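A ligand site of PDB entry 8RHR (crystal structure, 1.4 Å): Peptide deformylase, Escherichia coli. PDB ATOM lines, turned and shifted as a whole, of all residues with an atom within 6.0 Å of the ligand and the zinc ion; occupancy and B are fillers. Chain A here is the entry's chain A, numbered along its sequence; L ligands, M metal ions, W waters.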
ATOM      1  N   GLU A  45     -24.315 -27.340 -12.383  1.00  0.00           N
ATOM      2  CA  GLU A  45     -25.525 -26.541 -12.518  1.00  0.00           C
ATOM      3  C   GLU A  45     -25.490 -25.277 -11.667  1.00  0.00           C
ATOM      4  O   GLU A  45     -26.543 -24.813 -11.226  1.00  0.00           O
ATOM      5  CB  GLU A  45     -26.807 -27.366 -12.276  1.00  0.00           C
ATOM      6  CG  GLU A  45     -27.018 -28.589 -13.197  1.00  0.00           C
ATOM      7  CD  GLU A  45     -27.164 -28.317 -14.747  1.00  0.00           C
ATOM      8  OE1 GLU A  45     -27.401 -27.170 -15.182  1.00  0.00           O
ATOM      9  OE2 GLU A  45     -27.141 -29.316 -15.541  1.00  0.00           O
ATOM     10  N   GLY A  46     -24.260 -24.714 -11.475  1.00  0.00           N
ATOM     11  CA  GLY A  46     -24.046 -23.463 -10.779  1.00  0.00           C
ATOM     12  C   GLY A  46     -24.025 -22.247 -11.697  1.00  0.00           C
ATOM     13  O   GLY A  46     -23.884 -22.359 -12.924  1.00  0.00           O
ATOM     14  N   ILE A  47     -24.087 -21.068 -11.071  1.00  0.00           N
ATOM     15  CA  ILE A  47     -24.004 -19.801 -11.790  1.00  0.00           C
ATOM     16  C   ILE A  47     -22.696 -19.068 -11.519  1.00  0.00           C
ATOM     17  O   ILE A  47     -22.418 -18.046 -12.170  1.00  0.00           O
ATOM     18  CB  ILE A  47     -25.189 -18.864 -11.453  1.00  0.00           C
ATOM     19  CG1 ILE A  47     -25.228 -18.581  -9.936  1.00  0.00           C
ATOM     20  CG2 ILE A  47     -26.502 -19.527 -11.963  1.00  0.00           C
ATOM     21  CD1 ILE A  47     -26.104 -17.422  -9.544  1.00  0.00           C
ATOM     22  N   GLY A  48     -21.880 -19.575 -10.622  1.00  0.00           N
ATOM     23  CA  GLY A  48     -20.567 -18.999 -10.380  1.00  0.00           C
ATOM     24  C   GLY A  48     -19.666 -20.031  -9.751  1.00  0.00           C
ATOM     25  O   GLY A  48     -20.125 -21.010  -9.149  1.00  0.00           O
ATOM     26  N   LEU A  49     -18.367 -19.790  -9.888  1.00  0.00           N
ATOM     27  CA  LEU A  49     -17.367 -20.645  -9.217  1.00  0.00           C
ATOM     28  C   LEU A  49     -16.113 -19.839  -8.999  1.00  0.00           C
ATOM     29  O   LEU A  49     -15.645 -19.161  -9.920  1.00  0.00           O
ATOM     30  CB  LEU A  49     -17.061 -21.889 -10.081  1.00  0.00           C
ATOM     31  CG  LEU A  49     -16.275 -23.025  -9.476  1.00  0.00           C
ATOM     32  CD1 LEU A  49     -17.046 -23.686  -8.324  1.00  0.00           C
ATOM     33  CD2 LEU A  49     -15.878 -24.089 -10.492  1.00  0.00           C
ATOM     34  N   ALA A  50     -15.566 -19.927  -7.808  1.00  0.00           N
ATOM     35  CA  ALA A  50     -14.301 -19.292  -7.454  1.00  0.00           C
ATOM     36  C   ALA A  50     -13.216 -20.357  -7.389  1.00  0.00           C
ATOM     37  O   ALA A  50     -13.463 -21.506  -6.996  1.00  0.00           O
ATOM     38  CB  ALA A  50     -14.419 -18.540  -6.109  1.00  0.00           C
ATOM     39  N   GLN A  53     -12.860 -22.716  -4.490  1.00  0.00           N
ATOM     40  CA  GLN A  53     -13.769 -23.839  -4.342  1.00  0.00           C
ATOM     41  C   GLN A  53     -13.241 -25.102  -5.000  1.00  0.00           C
ATOM     42  O   GLN A  53     -13.734 -26.191  -4.697  1.00  0.00           O
ATOM     43  CB  GLN A  53     -15.134 -23.491  -4.937  1.00  0.00           C
ATOM     44  CG  GLN A  53     -15.927 -22.401  -4.187  1.00  0.00           C
ATOM     45  CD  GLN A  53     -17.207 -22.111  -4.899  1.00  0.00           C
ATOM     46  OE1 GLN A  53     -17.263 -21.271  -5.810  1.00  0.00           O
ATOM     47  NE2 GLN A  53     -18.246 -22.857  -4.563  1.00  0.00           N
ATOM     48  N   ILE A  89     -31.097 -12.195  -1.505  1.00  0.00           N
ATOM     49  CA  ILE A  89     -31.869 -13.346  -1.908  1.00  0.00           C
ATOM     50  C   ILE A  89     -31.424 -14.521  -1.036  1.00  0.00           C
ATOM     51  O   ILE A  89     -30.415 -14.445  -0.353  1.00  0.00           O
ATOM     52  CB  ILE A  89     -31.646 -13.690  -3.403  1.00  0.00           C
ATOM     53  CG1 ILE A  89     -30.206 -14.127  -3.683  1.00  0.00           C
ATOM     54  CG2 ILE A  89     -32.174 -12.537  -4.268  1.00  0.00           C
ATOM     55  CD1 ILE A  89     -29.946 -14.626  -5.146  1.00  0.00           C
ATOM     56  N   GLU A  90     -32.166 -15.623  -1.118  1.00  0.00           N
ATOM     57  CA  GLU A  90     -31.782 -16.880  -0.466  1.00  0.00           C
ATOM     58  C   GLU A  90     -30.707 -17.550  -1.337  1.00  0.00           C
ATOM     59  O   GLU A  90     -30.982 -18.251  -2.324  1.00  0.00           O
ATOM     60  CB  GLU A  90     -32.996 -17.765  -0.253  1.00  0.00           C
ATOM     61  CG  GLU A  90     -34.010 -17.180   0.739  1.00  0.00           C
ATOM     62  CD  GLU A  90     -35.096 -18.156   1.153  1.00  0.00           C
ATOM     63  OE1 GLU A  90     -35.188 -19.244   0.576  1.00  0.00           O
ATOM     64  OE2 GLU A  90     -35.825 -17.840   2.072  1.00  0.00           O
ATOM     65  N   GLU A  91     -29.453 -17.274  -1.001  1.00  0.00           N
ATOM     66  CA  GLU A  91     -28.311 -17.771  -1.750  1.00  0.00           C
ATOM     67  C   GLU A  91     -28.063 -19.220  -1.420  1.00  0.00           C
ATOM     68  O   GLU A  91     -28.317 -19.683  -0.301  1.00  0.00           O
ATOM     69  CB  GLU A  91     -27.059 -16.974  -1.379  1.00  0.00           C
ATOM     70  CG  GLU A  91     -27.106 -15.507  -1.813  1.00  0.00           C
ATOM     71  CD  GLU A  91     -25.831 -14.752  -1.558  1.00  0.00           C
ATOM     72  OE1 GLU A  91     -24.742 -15.351  -1.439  1.00  0.00           O
ATOM     73  OE2 GLU A  91     -25.919 -13.525  -1.418  1.00  0.00           O
ATOM     74  N   GLY A  92     -27.547 -19.923  -2.420  1.00  0.00           N
ATOM     75  CA  GLY A  92     -26.980 -21.242  -2.248  1.00  0.00           C
ATOM     76  C   GLY A  92     -25.516 -21.223  -2.611  1.00  0.00           C
ATOM     77  O   GLY A  92     -24.946 -20.152  -2.863  1.00  0.00           O
ATOM     78  N   CYS A  93     -24.881 -22.403  -2.626  1.00  0.00           N
ATOM     79  CA  CYS A  93     -23.453 -22.479  -2.908  1.00  0.00           C
ATOM     80  C   CYS A  93     -23.154 -23.928  -3.215  1.00  0.00           C
ATOM     81  O   CYS A  93     -23.563 -24.797  -2.445  1.00  0.00           O
ATOM     82  CB  CYS A  93     -22.610 -22.024  -1.713  1.00  0.00           C
ATOM     83  SG  CYS A  93     -20.817 -21.938  -2.074  1.00  0.00           S
ATOM     84  N   LEU A  94     -22.411 -24.172  -4.280  1.00  0.00           N
ATOM     85  CA  LEU A  94     -21.982 -25.541  -4.598  1.00  0.00           C
ATOM     86  C   LEU A  94     -21.183 -26.158  -3.456  1.00  0.00           C
ATOM     87  O   LEU A  94     -21.145 -27.373  -3.327  1.00  0.00           O
ATOM     88  CB  LEU A  94     -21.163 -25.591  -5.903  1.00  0.00           C
ATOM     89  CG  LEU A  94     -21.920 -25.260  -7.171  1.00  0.00           C
ATOM     90  CD1 LEU A  94     -20.949 -25.211  -8.389  1.00  0.00           C
ATOM     91  CD2 LEU A  94     -23.082 -26.248  -7.461  1.00  0.00           C
ATOM     92  N   SER A  95     -20.511 -25.335  -2.633  1.00  0.00           N
ATOM     93  CA  SER A  95     -19.715 -25.847  -1.518  1.00  0.00           C
ATOM     94  C   SER A  95     -20.546 -26.046  -0.250  1.00  0.00           C
ATOM     95  O   SER A  95     -20.016 -26.528   0.766  1.00  0.00           O
ATOM     96  CB  SER A  95     -18.528 -24.924  -1.207  1.00  0.00           C
ATOM     97  OG  SER A  95     -17.641 -24.775  -2.303  1.00  0.00           O
ATOM     98  N   LEU A 128     -29.200  -9.943  -9.713  1.00  0.00           N
ATOM     99  CA  LEU A 128     -28.570 -11.224  -9.434  1.00  0.00           C
ATOM    100  C   LEU A 128     -27.079 -11.186  -9.754  1.00  0.00           C
ATOM    101  O   LEU A 128     -26.275 -11.759  -9.014  1.00  0.00           O
ATOM    102  CB  LEU A 128     -29.271 -12.319 -10.240  1.00  0.00           C
ATOM    103  CG  LEU A 128     -28.676 -13.700 -10.177  1.00  0.00           C
ATOM    104  CD1 LEU A 128     -28.813 -14.256  -8.791  1.00  0.00           C
ATOM    105  CD2 LEU A 128     -29.371 -14.648 -11.155  1.00  0.00           C
ATOM    106  N   ILE A 131     -25.122  -9.697  -6.931  1.00  0.00           N
ATOM    107  CA  ILE A 131     -25.091 -10.612  -5.765  1.00  0.00           C
ATOM    108  C   ILE A 131     -24.072 -11.729  -6.028  1.00  0.00           C
ATOM    109  O   ILE A 131     -23.231 -12.049  -5.170  1.00  0.00           O
ATOM    110  CB  ILE A 131     -26.495 -11.169  -5.522  1.00  0.00           C
ATOM    111  CG1 ILE A 131     -27.402 -10.066  -4.967  1.00  0.00           C
ATOM    112  CG2 ILE A 131     -26.430 -12.388  -4.613  1.00  0.00           C
ATOM    113  CD1 ILE A 131     -28.844 -10.412  -5.011  1.00  0.00           C
ATOM    114  N   CYS A 132     -24.101 -12.295  -7.231  1.00  0.00           N
ATOM    115  CA  CYS A 132     -23.173 -13.380  -7.549  1.00  0.00           C
ATOM    116  C   CYS A 132     -21.697 -12.918  -7.551  1.00  0.00           C
ATOM    117  O   CYS A 132     -20.823 -13.607  -7.001  1.00  0.00           O
ATOM    118  CB  CYS A 132     -23.611 -13.943  -8.889  1.00  0.00           C
ATOM    119  SG  CYS A 132     -22.660 -15.363  -9.408  1.00  0.00           S
ATOM    120  N   HIS A 135     -20.722 -12.685  -3.860  1.00  0.00           N
ATOM    121  CA  HIS A 135     -20.572 -14.050  -3.335  1.00  0.00           C
ATOM    122  C   HIS A 135     -19.264 -14.687  -3.794  1.00  0.00           C
ATOM    123  O   HIS A 135     -18.519 -15.244  -2.979  1.00  0.00           O
ATOM    124  CB  HIS A 135     -21.811 -14.841  -3.763  1.00  0.00           C
ATOM    125  CG  HIS A 135     -21.788 -16.274  -3.371  1.00  0.00           C
ATOM    126  ND1 HIS A 135     -22.809 -16.857  -2.647  1.00  0.00           N
ATOM    127  CD2 HIS A 135     -20.963 -17.283  -3.737  1.00  0.00           C
ATOM    128  CE1 HIS A 135     -22.586 -18.158  -2.539  1.00  0.00           C
ATOM    129  NE2 HIS A 135     -21.464 -18.442  -3.161  1.00  0.00           N
ATOM    130  N   GLU A 136     -18.955 -14.578  -5.089  1.00  0.00           N
ATOM    131  CA  GLU A 136     -17.747 -15.201  -5.597  1.00  0.00           C
ATOM    132  C   GLU A 136     -16.490 -14.484  -5.111  1.00  0.00           C
ATOM    133  O   GLU A 136     -15.496 -15.136  -4.792  1.00  0.00           O
ATOM    134  CB  GLU A 136     -17.806 -15.316  -7.122  1.00  0.00           C
ATOM    135  CG  GLU A 136     -18.972 -16.116  -7.641  1.00  0.00           C
ATOM    136  CD  GLU A 136     -19.159 -17.479  -7.079  1.00  0.00           C
ATOM    137  OE1 GLU A 136     -18.173 -18.048  -6.628  1.00  0.00           O
ATOM    138  OE2 GLU A 136     -20.339 -17.975  -7.076  1.00  0.00           O
ATOM    139  N   HIS A 139     -15.553 -15.767  -1.750  1.00  0.00           N
ATOM    140  CA  HIS A 139     -14.839 -17.035  -1.741  1.00  0.00           C
ATOM    141  C   HIS A 139     -13.340 -16.820  -1.816  1.00  0.00           C
ATOM    142  O   HIS A 139     -12.577 -17.544  -1.188  1.00  0.00           O
ATOM    143  CB  HIS A 139     -15.265 -17.926  -2.909  1.00  0.00           C
ATOM    144  CG  HIS A 139     -16.515 -18.727  -2.712  1.00  0.00           C
ATOM    145  ND1 HIS A 139     -16.649 -19.642  -1.699  1.00  0.00           N
ATOM    146  CD2 HIS A 139     -17.641 -18.834  -3.468  1.00  0.00           C
ATOM    147  CE1 HIS A 139     -17.807 -20.267  -1.801  1.00  0.00           C
ATOM    148  NE2 HIS A 139     -18.452 -19.774  -2.841  1.00  0.00           N
ATOM    149  N   LEU A 144     -17.745 -17.412   3.218  1.00  0.00           N
ATOM    150  CA  LEU A 144     -18.876 -18.189   2.730  1.00  0.00           C
ATOM    151  C   LEU A 144     -20.169 -17.496   3.125  1.00  0.00           C
ATOM    152  O   LEU A 144     -20.224 -16.747   4.110  1.00  0.00           O
ATOM    153  CB  LEU A 144     -18.833 -19.607   3.350  1.00  0.00           C
ATOM    154  CG  LEU A 144     -17.561 -20.406   3.093  1.00  0.00           C
ATOM    155  CD1 LEU A 144     -17.620 -21.688   3.921  1.00  0.00           C
ATOM    156  CD2 LEU A 144     -17.441 -20.687   1.598  1.00  0.00           C
ATOM    157  N   PHE A 145     -21.255 -17.782   2.398  1.00  0.00           N
ATOM    158  CA  PHE A 145     -22.472 -17.031   2.656  1.00  0.00           C
ATOM    159  C   PHE A 145     -22.995 -17.271   4.055  1.00  0.00           C
ATOM    160  O   PHE A 145     -23.617 -16.385   4.668  1.00  0.00           O
ATOM    161  CB  PHE A 145     -23.562 -17.260   1.599  1.00  0.00           C
ATOM    162  CG  PHE A 145     -24.340 -18.536   1.767  1.00  0.00           C
ATOM    163  CD1 PHE A 145     -25.365 -18.653   2.706  1.00  0.00           C
ATOM    164  CD2 PHE A 145     -24.096 -19.615   0.924  1.00  0.00           C
ATOM    165  CE1 PHE A 145     -26.099 -19.836   2.814  1.00  0.00           C
ATOM    166  CE2 PHE A 145     -24.838 -20.800   1.044  1.00  0.00           C
ATOM    167  CZ  PHE A 145     -25.831 -20.906   1.986  1.00  0.00           C
HETATM  168 BR1  LIG L   1     -25.154 -15.811  -5.432  1.00  0.00          BR
HETATM  169  N1  LIG L   1     -20.785 -20.127  -5.629  1.00  0.00           N
HETATM  170  O1  LIG L   1     -21.056 -22.350  -5.943  1.00  0.00           O
HETATM  171  N2  LIG L   1     -25.864 -21.619  -6.228  1.00  0.00           N
HETATM  172  C1  LIG L   1     -24.618 -21.976  -6.665  1.00  0.00           C
HETATM  173  C2  LIG L   1     -23.823 -20.870  -6.709  1.00  0.00           C
HETATM  174  C3  LIG L   1     -24.625 -19.758  -6.265  1.00  0.00           C
HETATM  175  C4  LIG L   1     -24.393 -18.400  -6.102  1.00  0.00           C
HETATM  176  C5  LIG L   1     -25.456 -17.646  -5.649  1.00  0.00           C
HETATM  177  C6  LIG L   1     -26.734 -18.114  -5.377  1.00  0.00           C
HETATM  178  C7  LIG L   1     -26.979 -19.460  -5.554  1.00  0.00           C
HETATM  179  C8  LIG L   1     -25.912 -20.278  -5.974  1.00  0.00           C
HETATM  180  C9  LIG L   1     -22.407 -20.787  -7.123  1.00  0.00           C
HETATM  181  C10 LIG L   1     -21.373 -21.224  -6.148  1.00  0.00           C
HETATM  182  O2  LIG L   1     -19.521 -20.144  -5.133  1.00  0.00           O
HETATM  183 ZN    ZN M   1     -20.381 -20.216  -3.426  1.00  0.00          ZN
HETATM  184  O   HOH W   1     -26.685 -24.701  -7.226  1.00  0.00           O
HETATM  185  O   HOH W   2     -28.558 -22.909  -5.348  1.00  0.00           O
HETATM  186  O   HOH W   3     -30.156 -18.664  -4.889  1.00  0.00           O
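Gln 53 touches the zinc ion (NE2 to ZN, 3.6 Å).
The nearest printed residue that does not touch the zinc ion is Glu 136 (4.3 Å).
A ring nitrogen (ND1) of His 135 is in hydrogen-bond range of the side-chain carboxylate of Glu 91.
SG of Cys 93 sits close to NE2 of Gln 53, at 3.7 Å.
The side-chain sulfur (SG) of Cys 93 lies close to the backbone NH (N) of Ser 95, 3.5 Å away.
OE1 of Gln 53 lies close to OE1 of Glu 136 (3.4 Å).
NE2 of Gln 53 lies within hydrogen-bond range of OG of Ser 95, 3.0 Å away.
The backbone NH (N) of Ala 50 sits at hydrogen-bond distance from the side-chain amide oxygen (OE1) of Gln 53, at 2.9 Å.
The backbone NH of Ala 50 sits at hydrogen-bond distance from the side-chain carboxylate of Glu 136, at 3.4 Å.
The side-chain amide nitrogen (NE2) of Gln 53 is in hydrogen-bond range of an oxygen (O1) of the ligand.
A nitrogen (N1) of the ligand lies close to the side-chain carboxylate of Glu 136, 2.6 Å away.
N of Leu 94 is in hydrogen-bond range of O1 of the ligand (2.8 Å).
The zinc ion is bound by O2 of the ligand (1.9 Å), NE2 of His 139 (2.1 Å), NE2 of His 135 (2.1 Å) and SG of Cys 93 (2.2 Å).
The zinc ion has four donor atoms within binding distance.
Residues that only touch the ligand: Gly 48 (3.1 Å), Gly 92 (3.2 Å), Ile 131 (3.7 Å), Cys 132 (3.8 Å), Ile 47 (3.9 Å) and Glu 91 (3.97 Å).
Hydrophobic or aromatic side chains within 4 Å of the ligand: Ile 47, Leu 94, Ile 131, His 135 and His 139.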
